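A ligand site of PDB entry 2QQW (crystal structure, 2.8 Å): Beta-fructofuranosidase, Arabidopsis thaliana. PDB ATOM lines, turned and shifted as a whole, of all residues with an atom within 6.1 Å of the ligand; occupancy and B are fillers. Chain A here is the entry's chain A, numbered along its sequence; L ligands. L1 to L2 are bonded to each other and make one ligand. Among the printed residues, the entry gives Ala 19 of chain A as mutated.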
ATOM      1  N   TRP A  16     -18.283 -14.769  35.408  1.00  0.00           N
ATOM      2  CA  TRP A  16     -17.772 -13.491  34.935  1.00  0.00           C
ATOM      3  C   TRP A  16     -18.533 -12.285  35.481  1.00  0.00           C
ATOM      4  O   TRP A  16     -19.762 -12.258  35.480  1.00  0.00           O
ATOM      5  CB  TRP A  16     -17.814 -13.453  33.418  1.00  0.00           C
ATOM      6  CG  TRP A  16     -17.616 -12.070  32.858  1.00  0.00           C
ATOM      7  CD1 TRP A  16     -18.567 -11.098  32.671  1.00  0.00           C
ATOM      8  CD2 TRP A  16     -16.376 -11.488  32.432  1.00  0.00           C
ATOM      9  NE1 TRP A  16     -17.998  -9.960  32.151  1.00  0.00           N
ATOM     10  CE2 TRP A  16     -16.651 -10.168  32.001  1.00  0.00           C
ATOM     11  CE3 TRP A  16     -15.061 -11.944  32.371  1.00  0.00           C
ATOM     12  CZ2 TRP A  16     -15.669  -9.316  31.513  1.00  0.00           C
ATOM     13  CZ3 TRP A  16     -14.065 -11.091  31.886  1.00  0.00           C
ATOM     14  CH2 TRP A  16     -14.384  -9.800  31.467  1.00  0.00           C
ATOM     15  N   ASN A  18     -18.307  -7.814  35.140  1.00  0.00           N
ATOM     16  CA  ASN A  18     -17.718  -6.531  34.818  1.00  0.00           C
ATOM     17  C   ASN A  18     -18.469  -5.377  35.466  1.00  0.00           C
ATOM     18  O   ASN A  18     -18.758  -5.446  36.657  1.00  0.00           O
ATOM     19  CB  ASN A  18     -17.392  -6.335  33.311  1.00  0.00           C
ATOM     20  CG  ASN A  18     -18.603  -6.415  32.397  1.00  0.00           C
ATOM     21  OD1 ASN A  18     -19.233  -7.458  32.281  1.00  0.00           O
ATOM     22  ND2 ASN A  18     -18.911  -5.304  31.728  1.00  0.00           N
ATOM     23  N   ALA A  19     -18.811  -4.338  34.704  1.00  0.00           N
ATOM     24  CA  ALA A  19     -19.341  -3.077  35.211  1.00  0.00           C
ATOM     25  C   ALA A  19     -20.388  -3.205  36.320  1.00  0.00           C
ATOM     26  O   ALA A  19     -21.315  -4.025  36.203  1.00  0.00           O
ATOM     27  CB  ALA A  19     -19.908  -2.262  34.077  1.00  0.00           C
ATOM     28  N   GLN A  35     -23.148  -6.426  35.567  1.00  0.00           N
ATOM     29  CA  GLN A  35     -22.952  -7.224  34.378  1.00  0.00           C
ATOM     30  C   GLN A  35     -22.456  -8.624  34.755  1.00  0.00           C
ATOM     31  O   GLN A  35     -21.339  -8.784  35.251  1.00  0.00           O
ATOM     32  CB  GLN A  35     -21.963  -6.503  33.462  1.00  0.00           C
ATOM     33  CG  GLN A  35     -22.397  -5.114  33.049  1.00  0.00           C
ATOM     34  CD  GLN A  35     -23.503  -5.152  32.019  1.00  0.00           C
ATOM     35  OE1 GLN A  35     -23.305  -5.605  30.899  1.00  0.00           O
ATOM     36  NE2 GLN A  35     -24.675  -4.670  32.398  1.00  0.00           N
ATOM     37  N   TRP A  43     -16.583 -12.736  29.227  1.00  0.00           N
ATOM     38  CA  TRP A  43     -17.738 -11.896  28.887  1.00  0.00           C
ATOM     39  C   TRP A  43     -18.724 -12.650  27.968  1.00  0.00           C
ATOM     40  O   TRP A  43     -18.316 -13.277  26.995  1.00  0.00           O
ATOM     41  CB  TRP A  43     -17.278 -10.600  28.234  1.00  0.00           C
ATOM     42  CG  TRP A  43     -18.356  -9.562  28.170  1.00  0.00           C
ATOM     43  CD1 TRP A  43     -18.621  -8.605  29.101  1.00  0.00           C
ATOM     44  CD2 TRP A  43     -19.319  -9.394  27.124  1.00  0.00           C
ATOM     45  NE1 TRP A  43     -19.684  -7.836  28.695  1.00  0.00           N
ATOM     46  CE2 TRP A  43     -20.137  -8.298  27.480  1.00  0.00           C
ATOM     47  CE3 TRP A  43     -19.572 -10.060  25.908  1.00  0.00           C
ATOM     48  CZ2 TRP A  43     -21.187  -7.847  26.678  1.00  0.00           C
ATOM     49  CZ3 TRP A  43     -20.609  -9.608  25.110  1.00  0.00           C
ATOM     50  CH2 TRP A  43     -21.413  -8.515  25.501  1.00  0.00           C
ATOM     51  N   ILE A  46     -24.874 -11.444  28.743  1.00  0.00           N
ATOM     52  CA  ILE A  46     -24.769 -10.483  29.830  1.00  0.00           C
ATOM     53  C   ILE A  46     -26.119 -10.054  30.414  1.00  0.00           C
ATOM     54  O   ILE A  46     -26.967  -9.484  29.715  1.00  0.00           O
ATOM     55  CB  ILE A  46     -23.817  -9.306  29.461  1.00  0.00           C
ATOM     56  CG1 ILE A  46     -22.887  -8.994  30.624  1.00  0.00           C
ATOM     57  CG2 ILE A  46     -24.563  -8.087  28.935  1.00  0.00           C
ATOM     58  CD1 ILE A  46     -21.819 -10.105  30.877  1.00  0.00           C
ATOM     59  N   CYS A  77     -28.160  -7.057  27.813  1.00  0.00           N
ATOM     60  CA  CYS A  77     -28.550  -6.018  28.764  1.00  0.00           C
ATOM     61  C   CYS A  77     -27.318  -5.364  29.371  1.00  0.00           C
ATOM     62  O   CYS A  77     -26.844  -5.763  30.451  1.00  0.00           O
ATOM     63  CB  CYS A  77     -29.463  -6.596  29.834  1.00  0.00           C
ATOM     64  SG  CYS A  77     -31.039  -7.146  29.210  1.00  0.00           S
ATOM     65  N   TRP A  78     -26.818  -4.338  28.680  1.00  0.00           N
ATOM     66  CA  TRP A  78     -25.568  -3.663  29.035  1.00  0.00           C
ATOM     67  C   TRP A  78     -25.752  -2.647  30.163  1.00  0.00           C
ATOM     68  O   TRP A  78     -26.791  -2.623  30.829  1.00  0.00           O
ATOM     69  CB  TRP A  78     -24.953  -3.032  27.782  1.00  0.00           C
ATOM     70  CG  TRP A  78     -24.482  -4.037  26.786  1.00  0.00           C
ATOM     71  CD1 TRP A  78     -24.805  -5.367  26.746  1.00  0.00           C
ATOM     72  CD2 TRP A  78     -23.627  -3.797  25.661  1.00  0.00           C
ATOM     73  NE1 TRP A  78     -24.193  -5.970  25.681  1.00  0.00           N
ATOM     74  CE2 TRP A  78     -23.464  -5.038  24.998  1.00  0.00           C
ATOM     75  CE3 TRP A  78     -22.980  -2.670  25.153  1.00  0.00           C
ATOM     76  CZ2 TRP A  78     -22.677  -5.171  23.847  1.00  0.00           C
ATOM     77  CZ3 TRP A  78     -22.195  -2.807  24.011  1.00  0.00           C
ATOM     78  CH2 TRP A  78     -22.059  -4.055  23.372  1.00  0.00           C
ATOM     79  N   SER A  79     -24.739  -1.806  30.395  1.00  0.00           N
ATOM     80  CA  SER A  79     -24.740  -0.900  31.547  1.00  0.00           C
ATOM     81  C   SER A  79     -25.882   0.105  31.577  1.00  0.00           C
ATOM     82  O   SER A  79     -26.569   0.311  30.582  1.00  0.00           O
ATOM     83  CB  SER A  79     -23.408  -0.166  31.668  1.00  0.00           C
ATOM     84  OG  SER A  79     -22.422  -1.053  32.141  1.00  0.00           O
ATOM     85  N   GLY A  80     -26.042   0.713  32.737  1.00  0.00           N
ATOM     86  CA  GLY A  80     -27.123   1.655  32.985  1.00  0.00           C
ATOM     87  C   GLY A  80     -27.117   2.116  34.427  1.00  0.00           C
ATOM     88  O   GLY A  80     -26.287   1.682  35.223  1.00  0.00           O
ATOM     89  N   THR A  95     -28.883   0.235  28.491  1.00  0.00           N
ATOM     90  CA  THR A  95     -28.669   0.016  27.063  1.00  0.00           C
ATOM     91  C   THR A  95     -29.076  -1.415  26.732  1.00  0.00           C
ATOM     92  O   THR A  95     -28.688  -2.362  27.420  1.00  0.00           O
ATOM     93  CB  THR A  95     -27.195   0.266  26.668  1.00  0.00           C
ATOM     94  OG1 THR A  95     -26.845   1.645  26.900  1.00  0.00           O
ATOM     95  CG2 THR A  95     -26.938  -0.062  25.204  1.00  0.00           C
ATOM     96  N   GLN A 103     -27.324  -0.357  19.690  1.00  0.00           N
ATOM     97  CA  GLN A 103     -27.307   0.001  21.102  1.00  0.00           C
ATOM     98  C   GLN A 103     -28.378   1.038  21.414  1.00  0.00           C
ATOM     99  O   GLN A 103     -28.256   2.216  21.072  1.00  0.00           O
ATOM    100  CB  GLN A 103     -25.904   0.468  21.523  1.00  0.00           C
ATOM    101  CG  GLN A 103     -24.876  -0.656  21.563  1.00  0.00           C
ATOM    102  CD  GLN A 103     -23.436  -0.166  21.515  1.00  0.00           C
ATOM    103  OE1 GLN A 103     -23.152   1.026  21.655  1.00  0.00           O
ATOM    104  NE2 GLN A 103     -22.509  -1.109  21.324  1.00  0.00           N
ATOM    105  N   ARG A 144     -24.098   4.004  24.264  1.00  0.00           N
ATOM    106  CA  ARG A 144     -24.353   3.213  25.469  1.00  0.00           C
ATOM    107  C   ARG A 144     -24.107   3.868  26.833  1.00  0.00           C
ATOM    108  O   ARG A 144     -23.463   4.917  26.921  1.00  0.00           O
ATOM    109  CB  ARG A 144     -23.661   1.834  25.388  1.00  0.00           C
ATOM    110  CG  ARG A 144     -22.136   1.841  25.420  1.00  0.00           C
ATOM    111  CD  ARG A 144     -21.592   0.448  25.148  1.00  0.00           C
ATOM    112  NE  ARG A 144     -20.155   0.418  24.882  1.00  0.00           N
ATOM    113  CZ  ARG A 144     -19.602   0.604  23.695  1.00  0.00           C
ATOM    114  NH1 ARG A 144     -20.357   0.844  22.634  1.00  0.00           N
ATOM    115  NH2 ARG A 144     -18.284   0.563  23.554  1.00  0.00           N
ATOM    116  N   ASP A 145     -24.637   3.230  27.868  1.00  0.00           N
ATOM    117  CA  ASP A 145     -24.426   3.567  29.279  1.00  0.00           C
ATOM    118  C   ASP A 145     -25.033   4.906  29.681  1.00  0.00           C
ATOM    119  O   ASP A 145     -24.294   5.857  29.958  1.00  0.00           O
ATOM    120  CB  ASP A 145     -22.951   3.509  29.683  1.00  0.00           C
ATOM    121  CG  ASP A 145     -22.206   2.319  29.106  1.00  0.00           C
ATOM    122  OD1 ASP A 145     -22.844   1.286  28.817  1.00  0.00           O
ATOM    123  OD2 ASP A 145     -20.970   2.428  28.934  1.00  0.00           O
ATOM    124  N   MET A 197     -14.098   6.138  22.135  1.00  0.00           N
ATOM    125  CA  MET A 197     -15.397   5.884  22.763  1.00  0.00           C
ATOM    126  C   MET A 197     -15.425   6.292  24.242  1.00  0.00           C
ATOM    127  O   MET A 197     -14.524   5.928  25.017  1.00  0.00           O
ATOM    128  CB  MET A 197     -15.764   4.400  22.617  1.00  0.00           C
ATOM    129  CG  MET A 197     -17.060   4.003  23.296  1.00  0.00           C
ATOM    130  SD  MET A 197     -18.483   4.713  22.459  1.00  0.00           S
ATOM    131  CE  MET A 197     -19.708   4.398  23.718  1.00  0.00           C
ATOM    132  N   GLU A 199     -17.245   5.480  27.477  1.00  0.00           N
ATOM    133  CA  GLU A 199     -18.085   4.494  28.158  1.00  0.00           C
ATOM    134  C   GLU A 199     -18.402   4.970  29.562  1.00  0.00           C
ATOM    135  O   GLU A 199     -17.693   5.828  30.113  1.00  0.00           O
ATOM    136  CB  GLU A 199     -17.407   3.113  28.217  1.00  0.00           C
ATOM    137  CG  GLU A 199     -16.899   2.604  26.883  1.00  0.00           C
ATOM    138  CD  GLU A 199     -16.398   1.162  26.946  1.00  0.00           C
ATOM    139  OE1 GLU A 199     -16.572   0.443  25.934  1.00  0.00           O
ATOM    140  OE2 GLU A 199     -15.845   0.740  27.987  1.00  0.00           O
ATOM    141  N   CYS A 200     -19.448   4.401  30.144  1.00  0.00           N
ATOM    142  CA  CYS A 200     -19.856   4.679  31.533  1.00  0.00           C
ATOM    143  C   CYS A 200     -19.694   6.136  31.946  1.00  0.00           C
ATOM    144  O   CYS A 200     -18.970   6.425  32.891  1.00  0.00           O
ATOM    145  CB  CYS A 200     -19.109   3.791  32.509  1.00  0.00           C
ATOM    146  SG  CYS A 200     -19.297   2.061  32.175  1.00  0.00           S
ATOM    147  N   ASP A 235     -12.604   3.702  26.337  1.00  0.00           N
ATOM    148  CA  ASP A 235     -12.522   2.348  25.786  1.00  0.00           C
ATOM    149  C   ASP A 235     -11.118   2.005  25.271  1.00  0.00           C
ATOM    150  O   ASP A 235     -10.687   0.858  25.388  1.00  0.00           O
ATOM    151  CB  ASP A 235     -13.567   2.145  24.678  1.00  0.00           C
ATOM    152  CG  ASP A 235     -13.780   0.682  24.296  1.00  0.00           C
ATOM    153  OD1 ASP A 235     -14.367   0.429  23.229  1.00  0.00           O
ATOM    154  OD2 ASP A 235     -13.367  -0.221  25.063  1.00  0.00           O
ATOM    155  N   LYS A 238      -8.505   2.094  28.457  1.00  0.00           N
ATOM    156  CA  LYS A 238      -9.068   1.296  29.551  1.00  0.00           C
ATOM    157  C   LYS A 238      -8.890   1.922  30.932  1.00  0.00           C
ATOM    158  O   LYS A 238      -8.537   1.243  31.891  1.00  0.00           O
ATOM    159  CB  LYS A 238      -8.545  -0.156  29.526  1.00  0.00           C
ATOM    160  CG  LYS A 238      -9.527  -1.164  28.876  1.00  0.00           C
ATOM    161  CD  LYS A 238      -9.356  -1.272  27.332  1.00  0.00           C
ATOM    162  CE  LYS A 238     -10.415  -2.162  26.673  1.00  0.00           C
ATOM    163  NZ  LYS A 238     -11.790  -1.637  26.906  1.00  0.00           N
ATOM    164  N   TYR A 275     -11.883   0.241  36.440  1.00  0.00           N
ATOM    165  CA  TYR A 275     -12.660   0.606  35.240  1.00  0.00           C
ATOM    166  C   TYR A 275     -14.165   0.533  35.415  1.00  0.00           C
ATOM    167  O   TYR A 275     -14.670  -0.094  36.350  1.00  0.00           O
ATOM    168  CB  TYR A 275     -12.252  -0.274  34.061  1.00  0.00           C
ATOM    169  CG  TYR A 275     -12.675   0.265  32.719  1.00  0.00           C
ATOM    170  CD1 TYR A 275     -12.034   1.356  32.140  1.00  0.00           C
ATOM    171  CD2 TYR A 275     -13.729  -0.315  32.015  1.00  0.00           C
ATOM    172  CE1 TYR A 275     -12.425   1.842  30.894  1.00  0.00           C
ATOM    173  CE2 TYR A 275     -14.130   0.174  30.778  1.00  0.00           C
ATOM    174  CZ  TYR A 275     -13.473   1.249  30.229  1.00  0.00           C
ATOM    175  OH  TYR A 275     -13.862   1.735  29.005  1.00  0.00           O
ATOM    176  N   ALA A 276     -14.885   1.191  34.493  1.00  0.00           N
ATOM    177  CA  ALA A 276     -16.349   1.222  34.433  1.00  0.00           C
ATOM    178  C   ALA A 276     -17.019   1.678  35.733  1.00  0.00           C
ATOM    179  O   ALA A 276     -18.074   1.173  36.119  1.00  0.00           O
ATOM    180  CB  ALA A 276     -16.892  -0.125  33.966  1.00  0.00           C
ATOM    181  N   TRP A 293     -15.059  -1.408  38.975  1.00  0.00           N
ATOM    182  CA  TRP A 293     -14.738  -2.750  38.546  1.00  0.00           C
ATOM    183  C   TRP A 293     -13.226  -2.927  38.366  1.00  0.00           C
ATOM    184  O   TRP A 293     -12.596  -2.183  37.638  1.00  0.00           O
ATOM    185  CB  TRP A 293     -15.501  -3.069  37.249  1.00  0.00           C
ATOM    186  CG  TRP A 293     -15.052  -4.315  36.532  1.00  0.00           C
ATOM    187  CD1 TRP A 293     -14.882  -5.569  37.057  1.00  0.00           C
ATOM    188  CD2 TRP A 293     -14.739  -4.428  35.126  1.00  0.00           C
ATOM    189  NE1 TRP A 293     -14.467  -6.447  36.080  1.00  0.00           N
ATOM    190  CE2 TRP A 293     -14.379  -5.773  34.890  1.00  0.00           C
ATOM    191  CE3 TRP A 293     -14.745  -3.521  34.058  1.00  0.00           C
ATOM    192  CZ2 TRP A 293     -14.017  -6.237  33.623  1.00  0.00           C
ATOM    193  CZ3 TRP A 293     -14.384  -3.985  32.791  1.00  0.00           C
ATOM    194  CH2 TRP A 293     -14.032  -5.328  32.587  1.00  0.00           C
HETATM  195  C1  LIG L   1     -17.344  -3.230  27.800  1.00  0.00           C
HETATM  196  C2  LIG L   1     -15.989  -2.945  27.141  1.00  0.00           C
HETATM  197  C3  LIG L   1     -16.179  -2.546  25.668  1.00  0.00           C
HETATM  198  C4  LIG L   1     -17.038  -3.579  24.946  1.00  0.00           C
HETATM  199  C5  LIG L   1     -18.327  -3.802  25.722  1.00  0.00           C
HETATM  200  C6  LIG L   1     -19.221  -4.819  25.021  1.00  0.00           C
HETATM  201  O1  LIG L   1     -15.345  -1.900  27.835  1.00  0.00           O
HETATM  202  O2  LIG L   1     -14.938  -2.351  25.003  1.00  0.00           O
HETATM  203  O3  LIG L   1     -17.369  -3.158  23.641  1.00  0.00           O
HETATM  204  O4  LIG L   1     -18.055  -4.207  27.055  1.00  0.00           O
HETATM  205  O5  LIG L   1     -18.455  -5.814  24.388  1.00  0.00           O
HETATM  206  C1  LG2 L   2     -17.952  -1.135  30.142  1.00  0.00           C
HETATM  207  C2  LG2 L   2     -18.844  -1.791  29.097  1.00  0.00           C
HETATM  208  C3  LG2 L   2     -20.008  -0.882  28.794  1.00  0.00           C
HETATM  209  C4  LG2 L   2     -21.091  -1.835  28.369  1.00  0.00           C
HETATM  210  C5  LG2 L   2     -20.796  -3.043  29.248  1.00  0.00           C
HETATM  211  C6  LG2 L   2     -21.097  -4.386  28.579  1.00  0.00           C
HETATM  212  O1  LG2 L   2     -17.304  -2.153  30.877  1.00  0.00           O
HETATM  213  O2  LG2 L   2     -18.122  -2.029  27.899  1.00  0.00           O
HETATM  214  O3  LG2 L   2     -19.720   0.006  27.758  1.00  0.00           O
HETATM  215  O4  LG2 L   2     -22.340  -1.238  28.625  1.00  0.00           O
HETATM  216  O5  LG2 L   2     -19.429  -2.985  29.590  1.00  0.00           O
HETATM  217  O6  LG2 L   2     -20.867  -5.415  29.519  1.00  0.00           O
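The side-chain amide oxygen (OE1) of Gln 35 lies within hydrogen-bond range of an oxygen (O6) of LG2 L2. The side-chain carboxylate (OD1) of Asp 145 lies within hydrogen-bond range of an oxygen (O4) of LG2 L2, 2.6 Å away. The side-chain amide nitrogen (ND2) of Asn 18 sits at hydrogen-bond distance from an oxygen (O6) of LG2 L2 (3.0 Å). The guanidinium group (NE) of Arg 144 sits at hydrogen-bond distance from an oxygen (O3) of LG2 L2 (2.9 Å). N of Ser 79 is in hydrogen-bond range of O4 of LG2 L2 (3.0 Å). OD2 of Asp 235 lies within hydrogen-bond range of O2 of LIG L1 (2.6 Å). NE1 of Trp 43 lies within hydrogen-bond range of O6 of LG2 L2 (2.8 Å). The side-chain carboxylate of Glu 199 lies within hydrogen-bond range of an oxygen (O1) of LIG L1, at 2.7 Å.
The side-chain hydroxyl (OG1) of Thr 95 sits at hydrogen-bond distance from the backbone NH (N) of Asp 145 (2.9 Å). N of Asn 18 sits at hydrogen-bond distance from O of Gln 35. NE2 of Gln 35 sits close to N of Ser 79, at 3.5 Å. The guanidinium group (NH2) of Arg 144 is in salt-bridge range of the side-chain carboxylate (OE1) of Glu 199. The side-chain carboxylate (OD2) of Asp 145 lies within hydrogen-bond range of the backbone NH (N) of Cys 200, at 2.8 Å. N of Trp 78 lies within hydrogen-bond range of O of Thr 95 (3.0 Å). OD2 of Asp 235 lies within salt-bridge range of NZ of Lys 238, 2.8 Å away. The backbone carbonyl oxygen of Cys 77 lies within hydrogen-bond range of the side-chain amide nitrogen of Gln 35 (3.1 Å).
Residues that only touch the ligand: Trp 78 (3.3 Å), Lys 238 (3.7 Å), Tyr 275 (3.8 Å), Ala 276 (3.7 Å) and Trp 293 (3.9 Å). Hydrophobic or aromatic side chains within 4 Å of the ligand: Trp 43, Trp 78, Tyr 275, Ala 276 and Trp 293. Of the 22 residues printed, 13 come within 4 Å of the ligand.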
